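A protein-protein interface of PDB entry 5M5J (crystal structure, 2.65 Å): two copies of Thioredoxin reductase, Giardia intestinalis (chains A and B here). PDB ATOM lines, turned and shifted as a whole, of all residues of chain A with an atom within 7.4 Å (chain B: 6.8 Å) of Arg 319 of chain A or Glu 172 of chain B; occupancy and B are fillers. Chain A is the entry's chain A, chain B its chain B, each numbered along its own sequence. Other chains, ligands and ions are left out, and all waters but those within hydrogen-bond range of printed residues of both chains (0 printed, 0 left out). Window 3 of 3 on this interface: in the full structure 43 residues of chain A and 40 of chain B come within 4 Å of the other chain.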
ATOM      1  N   ILE A  20      18.325 -28.035  -4.173  1.00  0.00           N
ATOM      2  CA  ILE A  20      19.493 -27.173  -4.297  1.00  0.00           C
ATOM      3  C   ILE A  20      20.154 -27.400  -5.654  1.00  0.00           C
ATOM      4  O   ILE A  20      20.384 -28.542  -6.060  1.00  0.00           O
ATOM      5  CB  ILE A  20      20.500 -27.410  -3.150  1.00  0.00           C
ATOM      6  CG1 ILE A  20      19.759 -27.388  -1.795  1.00  0.00           C
ATOM      7  CG2 ILE A  20      21.602 -26.351  -3.189  1.00  0.00           C
ATOM      8  CD1 ILE A  20      20.630 -27.397  -0.554  1.00  0.00           C
ATOM      9  N   LEU A  41      18.154 -33.851   0.588  1.00  0.00           N
ATOM     10  CA  LEU A  41      17.593 -32.851  -0.307  1.00  0.00           C
ATOM     11  C   LEU A  41      17.961 -33.269  -1.713  1.00  0.00           C
ATOM     12  O   LEU A  41      19.093 -33.688  -1.956  1.00  0.00           O
ATOM     13  CB  LEU A  41      18.166 -31.475   0.007  1.00  0.00           C
ATOM     14  CG  LEU A  41      17.734 -30.919   1.366  1.00  0.00           C
ATOM     15  CD1 LEU A  41      18.718 -29.879   1.878  1.00  0.00           C
ATOM     16  CD2 LEU A  41      16.333 -30.331   1.282  1.00  0.00           C
ATOM     17  N   THR A 281      28.695 -15.843   6.709  1.00  0.00           N
ATOM     18  CA  THR A 281      27.910 -16.773   5.887  1.00  0.00           C
ATOM     19  C   THR A 281      28.360 -16.742   4.430  1.00  0.00           C
ATOM     20  O   THR A 281      29.211 -15.931   4.046  1.00  0.00           O
ATOM     21  CB  THR A 281      26.391 -16.484   5.943  1.00  0.00           C
ATOM     22  OG1 THR A 281      26.117 -15.210   5.341  1.00  0.00           O
ATOM     23  CG2 THR A 281      25.858 -16.522   7.388  1.00  0.00           C
ATOM     24  N   PHE A 290      23.628 -18.651  -2.859  1.00  0.00           N
ATOM     25  CA  PHE A 290      24.850 -18.680  -2.062  1.00  0.00           C
ATOM     26  C   PHE A 290      26.011 -18.963  -2.991  1.00  0.00           C
ATOM     27  O   PHE A 290      25.829 -19.594  -4.034  1.00  0.00           O
ATOM     28  CB  PHE A 290      24.734 -19.747  -0.975  1.00  0.00           C
ATOM     29  CG  PHE A 290      23.457 -19.649  -0.195  1.00  0.00           C
ATOM     30  CD1 PHE A 290      23.336 -18.740   0.855  1.00  0.00           C
ATOM     31  CD2 PHE A 290      22.352 -20.416  -0.547  1.00  0.00           C
ATOM     32  CE1 PHE A 290      22.148 -18.618   1.559  1.00  0.00           C
ATOM     33  CE2 PHE A 290      21.160 -20.299   0.154  1.00  0.00           C
ATOM     34  CZ  PHE A 290      21.059 -19.399   1.212  1.00  0.00           C
ATOM     35  N   LYS A 312      29.603 -24.761   4.307  1.00  0.00           N
ATOM     36  CA  LYS A 312      28.899 -23.593   4.858  1.00  0.00           C
ATOM     37  C   LYS A 312      27.742 -23.129   3.966  1.00  0.00           C
ATOM     38  O   LYS A 312      26.674 -22.774   4.466  1.00  0.00           O
ATOM     39  CB  LYS A 312      29.870 -22.431   5.098  1.00  0.00           C
ATOM     40  CG  LYS A 312      30.805 -22.662   6.271  1.00  0.00           C
ATOM     41  CD  LYS A 312      31.980 -21.702   6.269  1.00  0.00           C
ATOM     42  CE  LYS A 312      31.576 -20.306   6.702  1.00  0.00           C
ATOM     43  NZ  LYS A 312      32.661 -19.323   6.438  1.00  0.00           N
ATOM     44  N   ALA A 313      27.965 -23.148   2.655  1.00  0.00           N
ATOM     45  CA  ALA A 313      26.941 -22.784   1.680  1.00  0.00           C
ATOM     46  C   ALA A 313      25.740 -23.747   1.700  1.00  0.00           C
ATOM     47  O   ALA A 313      24.593 -23.300   1.723  1.00  0.00           O
ATOM     48  CB  ALA A 313      27.543 -22.724   0.284  1.00  0.00           C
ATOM     49  N   ALA A 314      26.015 -25.052   1.682  1.00  0.00           N
ATOM     50  CA  ALA A 314      24.965 -26.083   1.723  1.00  0.00           C
ATOM     51  C   ALA A 314      24.142 -26.052   3.022  1.00  0.00           C
ATOM     52  O   ALA A 314      22.942 -26.328   3.008  1.00  0.00           O
ATOM     53  CB  ALA A 314      25.570 -27.473   1.520  1.00  0.00           C
ATOM     54  N   LEU A 315      24.800 -25.731   4.135  1.00  0.00           N
ATOM     55  CA  LEU A 315      24.126 -25.537   5.417  1.00  0.00           C
ATOM     56  C   LEU A 315      23.319 -24.238   5.437  1.00  0.00           C
ATOM     57  O   LEU A 315      22.241 -24.203   6.018  1.00  0.00           O
ATOM     58  CB  LEU A 315      25.139 -25.538   6.567  1.00  0.00           C
ATOM     59  CG  LEU A 315      25.962 -26.824   6.732  1.00  0.00           C
ATOM     60  CD1 LEU A 315      27.132 -26.588   7.678  1.00  0.00           C
ATOM     61  CD2 LEU A 315      25.106 -27.990   7.206  1.00  0.00           C
ATOM     62  N   ASP A 316      23.838 -23.175   4.821  1.00  0.00           N
ATOM     63  CA  ASP A 316      23.066 -21.928   4.647  1.00  0.00           C
ATOM     64  C   ASP A 316      21.791 -22.158   3.817  1.00  0.00           C
ATOM     65  O   ASP A 316      20.743 -21.573   4.093  1.00  0.00           O
ATOM     66  CB  ASP A 316      23.906 -20.832   3.970  1.00  0.00           C
ATOM     67  CG  ASP A 316      25.015 -20.283   4.855  1.00  0.00           C
ATOM     68  OD1 ASP A 316      24.983 -20.467   6.090  1.00  0.00           O
ATOM     69  OD2 ASP A 316      25.931 -19.645   4.296  1.00  0.00           O
ATOM     70  N   ALA A 317      21.895 -23.005   2.800  1.00  0.00           N
ATOM     71  CA  ALA A 317      20.777 -23.315   1.928  1.00  0.00           C
ATOM     72  C   ALA A 317      19.701 -24.129   2.644  1.00  0.00           C
ATOM     73  O   ALA A 317      18.510 -23.860   2.490  1.00  0.00           O
ATOM     74  CB  ALA A 317      21.275 -24.059   0.695  1.00  0.00           C
ATOM     75  N   GLU A 318      20.125 -25.127   3.412  1.00  0.00           N
ATOM     76  CA  GLU A 318      19.202 -25.981   4.161  1.00  0.00           C
ATOM     77  C   GLU A 318      18.435 -25.177   5.209  1.00  0.00           C
ATOM     78  O   GLU A 318      17.218 -25.326   5.356  1.00  0.00           O
ATOM     79  CB  GLU A 318      19.969 -27.108   4.844  1.00  0.00           C
ATOM     80  CG  GLU A 318      19.083 -28.137   5.535  1.00  0.00           C
ATOM     81  CD  GLU A 318      19.870 -29.214   6.261  1.00  0.00           C
ATOM     82  OE1 GLU A 318      19.252 -30.238   6.634  1.00  0.00           O
ATOM     83  OE2 GLU A 318      21.095 -29.043   6.472  1.00  0.00           O
ATOM     84  N   ARG A 319      19.177 -24.341   5.931  1.00  0.00           N
ATOM     85  CA  ARG A 319      18.622 -23.421   6.911  1.00  0.00           C
ATOM     86  C   ARG A 319      17.596 -22.501   6.251  1.00  0.00           C
ATOM     87  O   ARG A 319      16.476 -22.344   6.747  1.00  0.00           O
ATOM     88  CB  ARG A 319      19.750 -22.598   7.552  1.00  0.00           C
ATOM     89  CG  ARG A 319      19.333 -21.764   8.760  1.00  0.00           C
ATOM     90  CD  ARG A 319      20.512 -21.152   9.515  1.00  0.00           C
ATOM     91  NE  ARG A 319      21.413 -22.173  10.072  1.00  0.00           N
ATOM     92  CZ  ARG A 319      22.601 -22.541   9.572  1.00  0.00           C
ATOM     93  NH1 ARG A 319      23.107 -21.987   8.460  1.00  0.00           N
ATOM     94  NH2 ARG A 319      23.303 -23.493  10.198  1.00  0.00           N
ATOM     95  N   TRP A 320      17.983 -21.912   5.123  1.00  0.00           N
ATOM     96  CA  TRP A 320      17.109 -21.020   4.357  1.00  0.00           C
ATOM     97  C   TRP A 320      15.847 -21.735   3.851  1.00  0.00           C
ATOM     98  O   TRP A 320      14.765 -21.150   3.868  1.00  0.00           O
ATOM     99  CB  TRP A 320      17.890 -20.406   3.193  1.00  0.00           C
ATOM    100  CG  TRP A 320      17.131 -19.399   2.418  1.00  0.00           C
ATOM    101  CD1 TRP A 320      16.890 -18.108   2.768  1.00  0.00           C
ATOM    102  CD2 TRP A 320      16.511 -19.596   1.145  1.00  0.00           C
ATOM    103  NE1 TRP A 320      16.145 -17.483   1.799  1.00  0.00           N
ATOM    104  CE2 TRP A 320      15.897 -18.372   0.789  1.00  0.00           C
ATOM    105  CE3 TRP A 320      16.404 -20.694   0.271  1.00  0.00           C
ATOM    106  CZ2 TRP A 320      15.196 -18.205  -0.408  1.00  0.00           C
ATOM    107  CZ3 TRP A 320      15.706 -20.531  -0.924  1.00  0.00           C
ATOM    108  CH2 TRP A 320      15.110 -19.288  -1.253  1.00  0.00           C
ATOM    109  N   LEU A 321      15.987 -22.990   3.422  1.00  0.00           N
ATOM    110  CA  LEU A 321      14.842 -23.789   2.956  1.00  0.00           C
ATOM    111  C   LEU A 321      13.806 -24.165   4.043  1.00  0.00           C
ATOM    112  O   LEU A 321      12.645 -24.418   3.709  1.00  0.00           O
ATOM    113  CB  LEU A 321      15.309 -25.050   2.204  1.00  0.00           C
ATOM    114  CG  LEU A 321      15.941 -24.823   0.824  1.00  0.00           C
ATOM    115  CD1 LEU A 321      16.471 -26.132   0.253  1.00  0.00           C
ATOM    116  CD2 LEU A 321      14.967 -24.169  -0.146  1.00  0.00           C
ATOM    117  N   ALA A 322      14.210 -24.217   5.318  1.00  0.00           N
ATOM    118  CA  ALA A 322      13.240 -24.224   6.427  1.00  0.00           C
ATOM    119  C   ALA A 322      12.684 -22.801   6.555  1.00  0.00           C
ATOM    120  O   ALA A 322      13.126 -22.010   7.396  1.00  0.00           O
ATOM    121  CB  ALA A 322      13.895 -24.676   7.717  1.00  0.00           C
ATOM    122  N   MET A 323      11.719 -22.489   5.690  1.00  0.00           N
ATOM    123  CA  MET A 323      11.349 -21.099   5.378  1.00  0.00           C
ATOM    124  C   MET A 323      10.806 -20.332   6.574  1.00  0.00           C
ATOM    125  O   MET A 323      11.421 -19.361   7.004  1.00  0.00           O
ATOM    126  CB  MET A 323      10.337 -21.044   4.219  1.00  0.00           C
ATOM    127  CG  MET A 323      10.928 -21.329   2.841  1.00  0.00           C
ATOM    128  SD  MET A 323      11.944 -19.993   2.155  1.00  0.00           S
ATOM    129  CE  MET A 323      11.975 -20.471   0.428  1.00  0.00           C
ATOM    130  N   ALA B 149      17.388 -31.155  15.381  1.00  0.00           N
ATOM    131  CA  ALA B 149      15.933 -31.150  15.169  1.00  0.00           C
ATOM    132  C   ALA B 149      15.532 -31.426  13.728  1.00  0.00           C
ATOM    133  O   ALA B 149      14.565 -32.144  13.486  1.00  0.00           O
ATOM    134  CB  ALA B 149      15.312 -29.844  15.641  1.00  0.00           C
ATOM    135  N   GLY B 167      19.134 -20.346  23.760  1.00  0.00           N
ATOM    136  CA  GLY B 167      20.230 -19.802  23.000  1.00  0.00           C
ATOM    137  C   GLY B 167      19.806 -19.837  21.557  1.00  0.00           C
ATOM    138  O   GLY B 167      18.716 -20.298  21.236  1.00  0.00           O
ATOM    139  N   ASP B 168      20.669 -19.352  20.681  1.00  0.00           N
ATOM    140  CA  ASP B 168      20.369 -19.320  19.264  1.00  0.00           C
ATOM    141  C   ASP B 168      20.129 -20.709  18.689  1.00  0.00           C
ATOM    142  O   ASP B 168      19.208 -20.903  17.906  1.00  0.00           O
ATOM    143  CB  ASP B 168      21.526 -18.648  18.535  1.00  0.00           C
ATOM    144  CG  ASP B 168      22.035 -17.436  19.272  1.00  0.00           C
ATOM    145  OD1 ASP B 168      21.467 -16.344  19.083  1.00  0.00           O
ATOM    146  OD2 ASP B 168      22.998 -17.578  20.050  1.00  0.00           O
ATOM    147  N   VAL B 169      20.937 -21.683  19.074  1.00  0.00           N
ATOM    148  CA  VAL B 169      20.729 -23.027  18.548  1.00  0.00           C
ATOM    149  C   VAL B 169      19.304 -23.460  18.910  1.00  0.00           C
ATOM    150  O   VAL B 169      18.507 -23.752  18.020  1.00  0.00           O
ATOM    151  CB  VAL B 169      21.790 -24.033  19.071  1.00  0.00           C
ATOM    152  CG1 VAL B 169      21.509 -25.446  18.560  1.00  0.00           C
ATOM    153  CG2 VAL B 169      23.194 -23.598  18.652  1.00  0.00           C
ATOM    154  N   ALA B 170      18.983 -23.438  20.204  1.00  0.00           N
ATOM    155  CA  ALA B 170      17.674 -23.889  20.702  1.00  0.00           C
ATOM    156  C   ALA B 170      16.491 -23.051  20.207  1.00  0.00           C
ATOM    157  O   ALA B 170      15.441 -23.612  19.891  1.00  0.00           O
ATOM    158  CB  ALA B 170      17.669 -23.926  22.218  1.00  0.00           C
ATOM    159  N   CYS B 171      16.657 -21.726  20.156  1.00  0.00           N
ATOM    160  CA  CYS B 171      15.581 -20.819  19.702  1.00  0.00           C
ATOM    161  C   CYS B 171      15.173 -21.069  18.244  1.00  0.00           C
ATOM    162  O   CYS B 171      13.995 -20.956  17.910  1.00  0.00           O
ATOM    163  CB  CYS B 171      15.963 -19.335  19.885  1.00  0.00           C
ATOM    164  SG  CYS B 171      15.924 -18.691  21.583  1.00  0.00           S
ATOM    165  N   GLU B 172      16.143 -21.394  17.388  1.00  0.00           N
ATOM    166  CA  GLU B 172      15.861 -21.768  15.989  1.00  0.00           C
ATOM    167  C   GLU B 172      15.292 -23.189  15.841  1.00  0.00           C
ATOM    168  O   GLU B 172      14.527 -23.446  14.909  1.00  0.00           O
ATOM    169  CB  GLU B 172      17.102 -21.595  15.096  1.00  0.00           C
ATOM    170  CG  GLU B 172      17.523 -20.136  14.907  1.00  0.00           C
ATOM    171  CD  GLU B 172      18.284 -19.854  13.612  1.00  0.00           C
ATOM    172  OE1 GLU B 172      18.451 -20.759  12.761  1.00  0.00           O
ATOM    173  OE2 GLU B 172      18.715 -18.693  13.439  1.00  0.00           O
ATOM    174  N   GLU B 173      15.672 -24.102  16.740  1.00  0.00           N
ATOM    175  CA  GLU B 173      15.119 -25.470  16.758  1.00  0.00           C
ATOM    176  C   GLU B 173      13.626 -25.441  17.094  1.00  0.00           C
ATOM    177  O   GLU B 173      12.825 -26.117  16.446  1.00  0.00           O
ATOM    178  CB  GLU B 173      15.835 -26.360  17.789  1.00  0.00           C
ATOM    179  CG  GLU B 173      17.343 -26.515  17.604  1.00  0.00           C
ATOM    180  CD  GLU B 173      17.752 -27.806  16.937  1.00  0.00           C
ATOM    181  OE1 GLU B 173      18.128 -28.762  17.655  1.00  0.00           O
ATOM    182  OE2 GLU B 173      17.705 -27.856  15.691  1.00  0.00           O
ATOM    183  N   ALA B 174      13.275 -24.651  18.110  1.00  0.00           N
ATOM    184  CA  ALA B 174      11.890 -24.501  18.569  1.00  0.00           C
ATOM    185  C   ALA B 174      10.958 -23.858  17.529  1.00  0.00           C
ATOM    186  O   ALA B 174       9.849 -24.354  17.311  1.00  0.00           O
ATOM    187  CB  ALA B 174      11.845 -23.713  19.872  1.00  0.00           C
ATOM    188  N   THR B 175      11.399 -22.766  16.901  1.00  0.00           N
ATOM    189  CA  THR B 175      10.604 -22.095  15.850  1.00  0.00           C
ATOM    190  C   THR B 175      10.402 -22.989  14.619  1.00  0.00           C
ATOM    191  O   THR B 175       9.351 -22.927  13.985  1.00  0.00           O
ATOM    192  CB  THR B 175      11.219 -20.746  15.406  1.00  0.00           C
ATOM    193  OG1 THR B 175      12.646 -20.852  15.353  1.00  0.00           O
ATOM    194  CG2 THR B 175      10.852 -19.638  16.368  1.00  0.00           C
ATOM    195  N   TYR B 176      11.404 -23.808  14.294  1.00  0.00           N
ATOM    196  CA  TYR B 176      11.283 -24.804  13.220  1.00  0.00           C
ATOM    197  C   TYR B 176      10.297 -25.928  13.573  1.00  0.00           C
ATOM    198  O   TYR B 176       9.457 -26.300  12.750  1.00  0.00           O
ATOM    199  CB  TYR B 176      12.647 -25.413  12.857  1.00  0.00           C
ATOM    200  CG  TYR B 176      12.528 -26.501  11.813  1.00  0.00           C
ATOM    201  CD1 TYR B 176      12.112 -26.197  10.512  1.00  0.00           C
ATOM    202  CD2 TYR B 176      12.781 -27.836  12.132  1.00  0.00           C
ATOM    203  CE1 TYR B 176      11.975 -27.189   9.552  1.00  0.00           C
ATOM    204  CE2 TYR B 176      12.652 -28.836  11.178  1.00  0.00           C
ATOM    205  CZ  TYR B 176      12.248 -28.508   9.888  1.00  0.00           C
ATOM    206  OH  TYR B 176      12.111 -29.493   8.934  1.00  0.00           O
ATOM    207  N   LEU B 177      10.406 -26.460  14.789  1.00  0.00           N
ATOM    208  CA  LEU B 177       9.534 -27.555  15.239  1.00  0.00           C
ATOM    209  C   LEU B 177       8.057 -27.157  15.459  1.00  0.00           C
ATOM    210  O   LEU B 177       7.217 -28.044  15.603  1.00  0.00           O
ATOM    211  CB  LEU B 177      10.119 -28.236  16.487  1.00  0.00           C
ATOM    212  CG  LEU B 177      11.442 -28.987  16.258  1.00  0.00           C
ATOM    213  CD1 LEU B 177      12.145 -29.278  17.576  1.00  0.00           C
ATOM    214  CD2 LEU B 177      11.225 -30.275  15.476  1.00  0.00           C
ATOM    215  N   MET B 186      10.175 -25.301  25.731  1.00  0.00           N
ATOM    216  CA  MET B 186      11.559 -24.826  25.923  1.00  0.00           C
ATOM    217  C   MET B 186      11.952 -24.772  27.403  1.00  0.00           C
ATOM    218  O   MET B 186      11.385 -23.988  28.170  1.00  0.00           O
ATOM    219  CB  MET B 186      11.744 -23.446  25.306  1.00  0.00           C
ATOM    220  CG  MET B 186      11.605 -23.425  23.796  1.00  0.00           C
ATOM    221  SD  MET B 186      12.347 -21.941  23.093  1.00  0.00           S
ATOM    222  CE  MET B 186      14.072 -22.417  23.076  1.00  0.00           C
ATOM    223  N   MET B 199      15.616 -13.157  17.977  1.00  0.00           N
ATOM    224  CA  MET B 199      15.250 -14.566  18.160  1.00  0.00           C
ATOM    225  C   MET B 199      14.325 -14.788  19.370  1.00  0.00           C
ATOM    226  O   MET B 199      13.451 -15.656  19.321  1.00  0.00           O
ATOM    227  CB  MET B 199      16.505 -15.456  18.261  1.00  0.00           C
ATOM    228  CG  MET B 199      16.372 -16.755  17.484  1.00  0.00           C
ATOM    229  SD  MET B 199      16.419 -16.498  15.695  1.00  0.00           S
ATOM    230  CE  MET B 199      14.860 -17.227  15.190  1.00  0.00           C
ATOM    231  N   VAL B 203      10.464 -16.290  19.417  1.00  0.00           N
ATOM    232  CA  VAL B 203      10.148 -17.329  20.411  1.00  0.00           C
ATOM    233  C   VAL B 203       9.003 -16.912  21.348  1.00  0.00           C
ATOM    234  O   VAL B 203       8.042 -17.664  21.526  1.00  0.00           O
ATOM    235  CB  VAL B 203      11.422 -17.726  21.214  1.00  0.00           C
ATOM    236  CG1 VAL B 203      11.100 -18.489  22.495  1.00  0.00           C
ATOM    237  CG2 VAL B 203      12.340 -18.559  20.333  1.00  0.00           C
ATOM    238  N   LEU B 299      27.935 -21.698  14.548  1.00  0.00           N
ATOM    239  CA  LEU B 299      26.904 -21.893  13.515  1.00  0.00           C
ATOM    240  C   LEU B 299      27.021 -23.211  12.763  1.00  0.00           C
ATOM    241  O   LEU B 299      26.023 -23.908  12.581  1.00  0.00           O
ATOM    242  CB  LEU B 299      26.940 -20.743  12.497  1.00  0.00           C
ATOM    243  CG  LEU B 299      26.722 -19.318  13.030  1.00  0.00           C
ATOM    244  CD1 LEU B 299      27.065 -18.263  11.982  1.00  0.00           C
ATOM    245  CD2 LEU B 299      25.290 -19.145  13.522  1.00  0.00           C
ATOM    246  N   TYR B 300      28.236 -23.552  12.340  1.00  0.00           N
ATOM    247  CA  TYR B 300      28.457 -24.632  11.368  1.00  0.00           C
ATOM    248  C   TYR B 300      28.946 -25.913  12.007  1.00  0.00           C
ATOM    249  O   TYR B 300      28.344 -26.970  11.823  1.00  0.00           O
ATOM    250  CB  TYR B 300      29.434 -24.162  10.281  1.00  0.00           C
ATOM    251  CG  TYR B 300      28.911 -22.943   9.570  1.00  0.00           C
ATOM    252  CD1 TYR B 300      27.787 -23.029   8.750  1.00  0.00           C
ATOM    253  CD2 TYR B 300      29.493 -21.692   9.753  1.00  0.00           C
ATOM    254  CE1 TYR B 300      27.272 -21.911   8.112  1.00  0.00           C
ATOM    255  CE2 TYR B 300      28.987 -20.567   9.116  1.00  0.00           C
ATOM    256  CZ  TYR B 300      27.876 -20.685   8.298  1.00  0.00           C
ATOM    257  OH  TYR B 300      27.355 -19.591   7.657  1.00  0.00           O
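NH1 of Arg 319 of chain A sits close to O of Leu 315 of chain A (3.4 Å). The side-chain carboxylate (OD1) of Asp 316 of chain A is in salt-bridge range of the guanidinium group (NH1) of Arg 319 of chain A (3.4 Å). OG1 of Thr 175 of chain B is in hydrogen-bond range of O of Glu 172 of chain B (3.2 Å).
Of the printed residues of chain B, Thr 281 of chain A touches Tyr 300. Printed residues of chain B within 4 Å of Lys 312 of chain A: Tyr 300. Ala 313 of chain A touches none of the printed residues of chain B. Printed residues of chain B within 4 Å of Leu 315 of chain A: Tyr 300. Arg 319 of chain A touches just these residues of chain B: Glu 172 and Leu 299. Of chain A, only Arg 319 comes within 4 Å of Glu 172 of chain B. Leu 177 of chain B touches none of the printed residues of chain A. The nearest residue of chain B that does not touch Arg 319 of chain A is Tyr 300 of chain B (4.2 Å).
Tyr 300 of chain B touches Thr 281 of chain A (OH to CA, 3.4 Å). Tyr 300 of chain B touches Lys 312 of chain A. CD1 of Leu 315 of chain A touches CD1 of Tyr 300 of chain B, 3.8 Å away. CD of Arg 319 of chain A touches OE1 of Glu 172 of chain B (3.9 Å). Arg 319 of chain A touches Leu 299 of chain B (NH2 to O, 3.6 Å). Ala 322 of chain A touches Tyr 176 of chain B (CB to CD1, 3.6 Å).
Of the 16 printed residues of chain A, 6 touch a printed residue of chain B. Of the 17 printed residues of chain B, 4 touch a printed residue of chain A. Hydrophobic or aromatic side chains of chain B within 4 Å of the printed part of chain A: Tyr 176 and Tyr 300.
OD1 of Asp 316 of chain A is in hydrogen-bond range of OH of Tyr 300 of chain B.
No position is printed for both chains.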
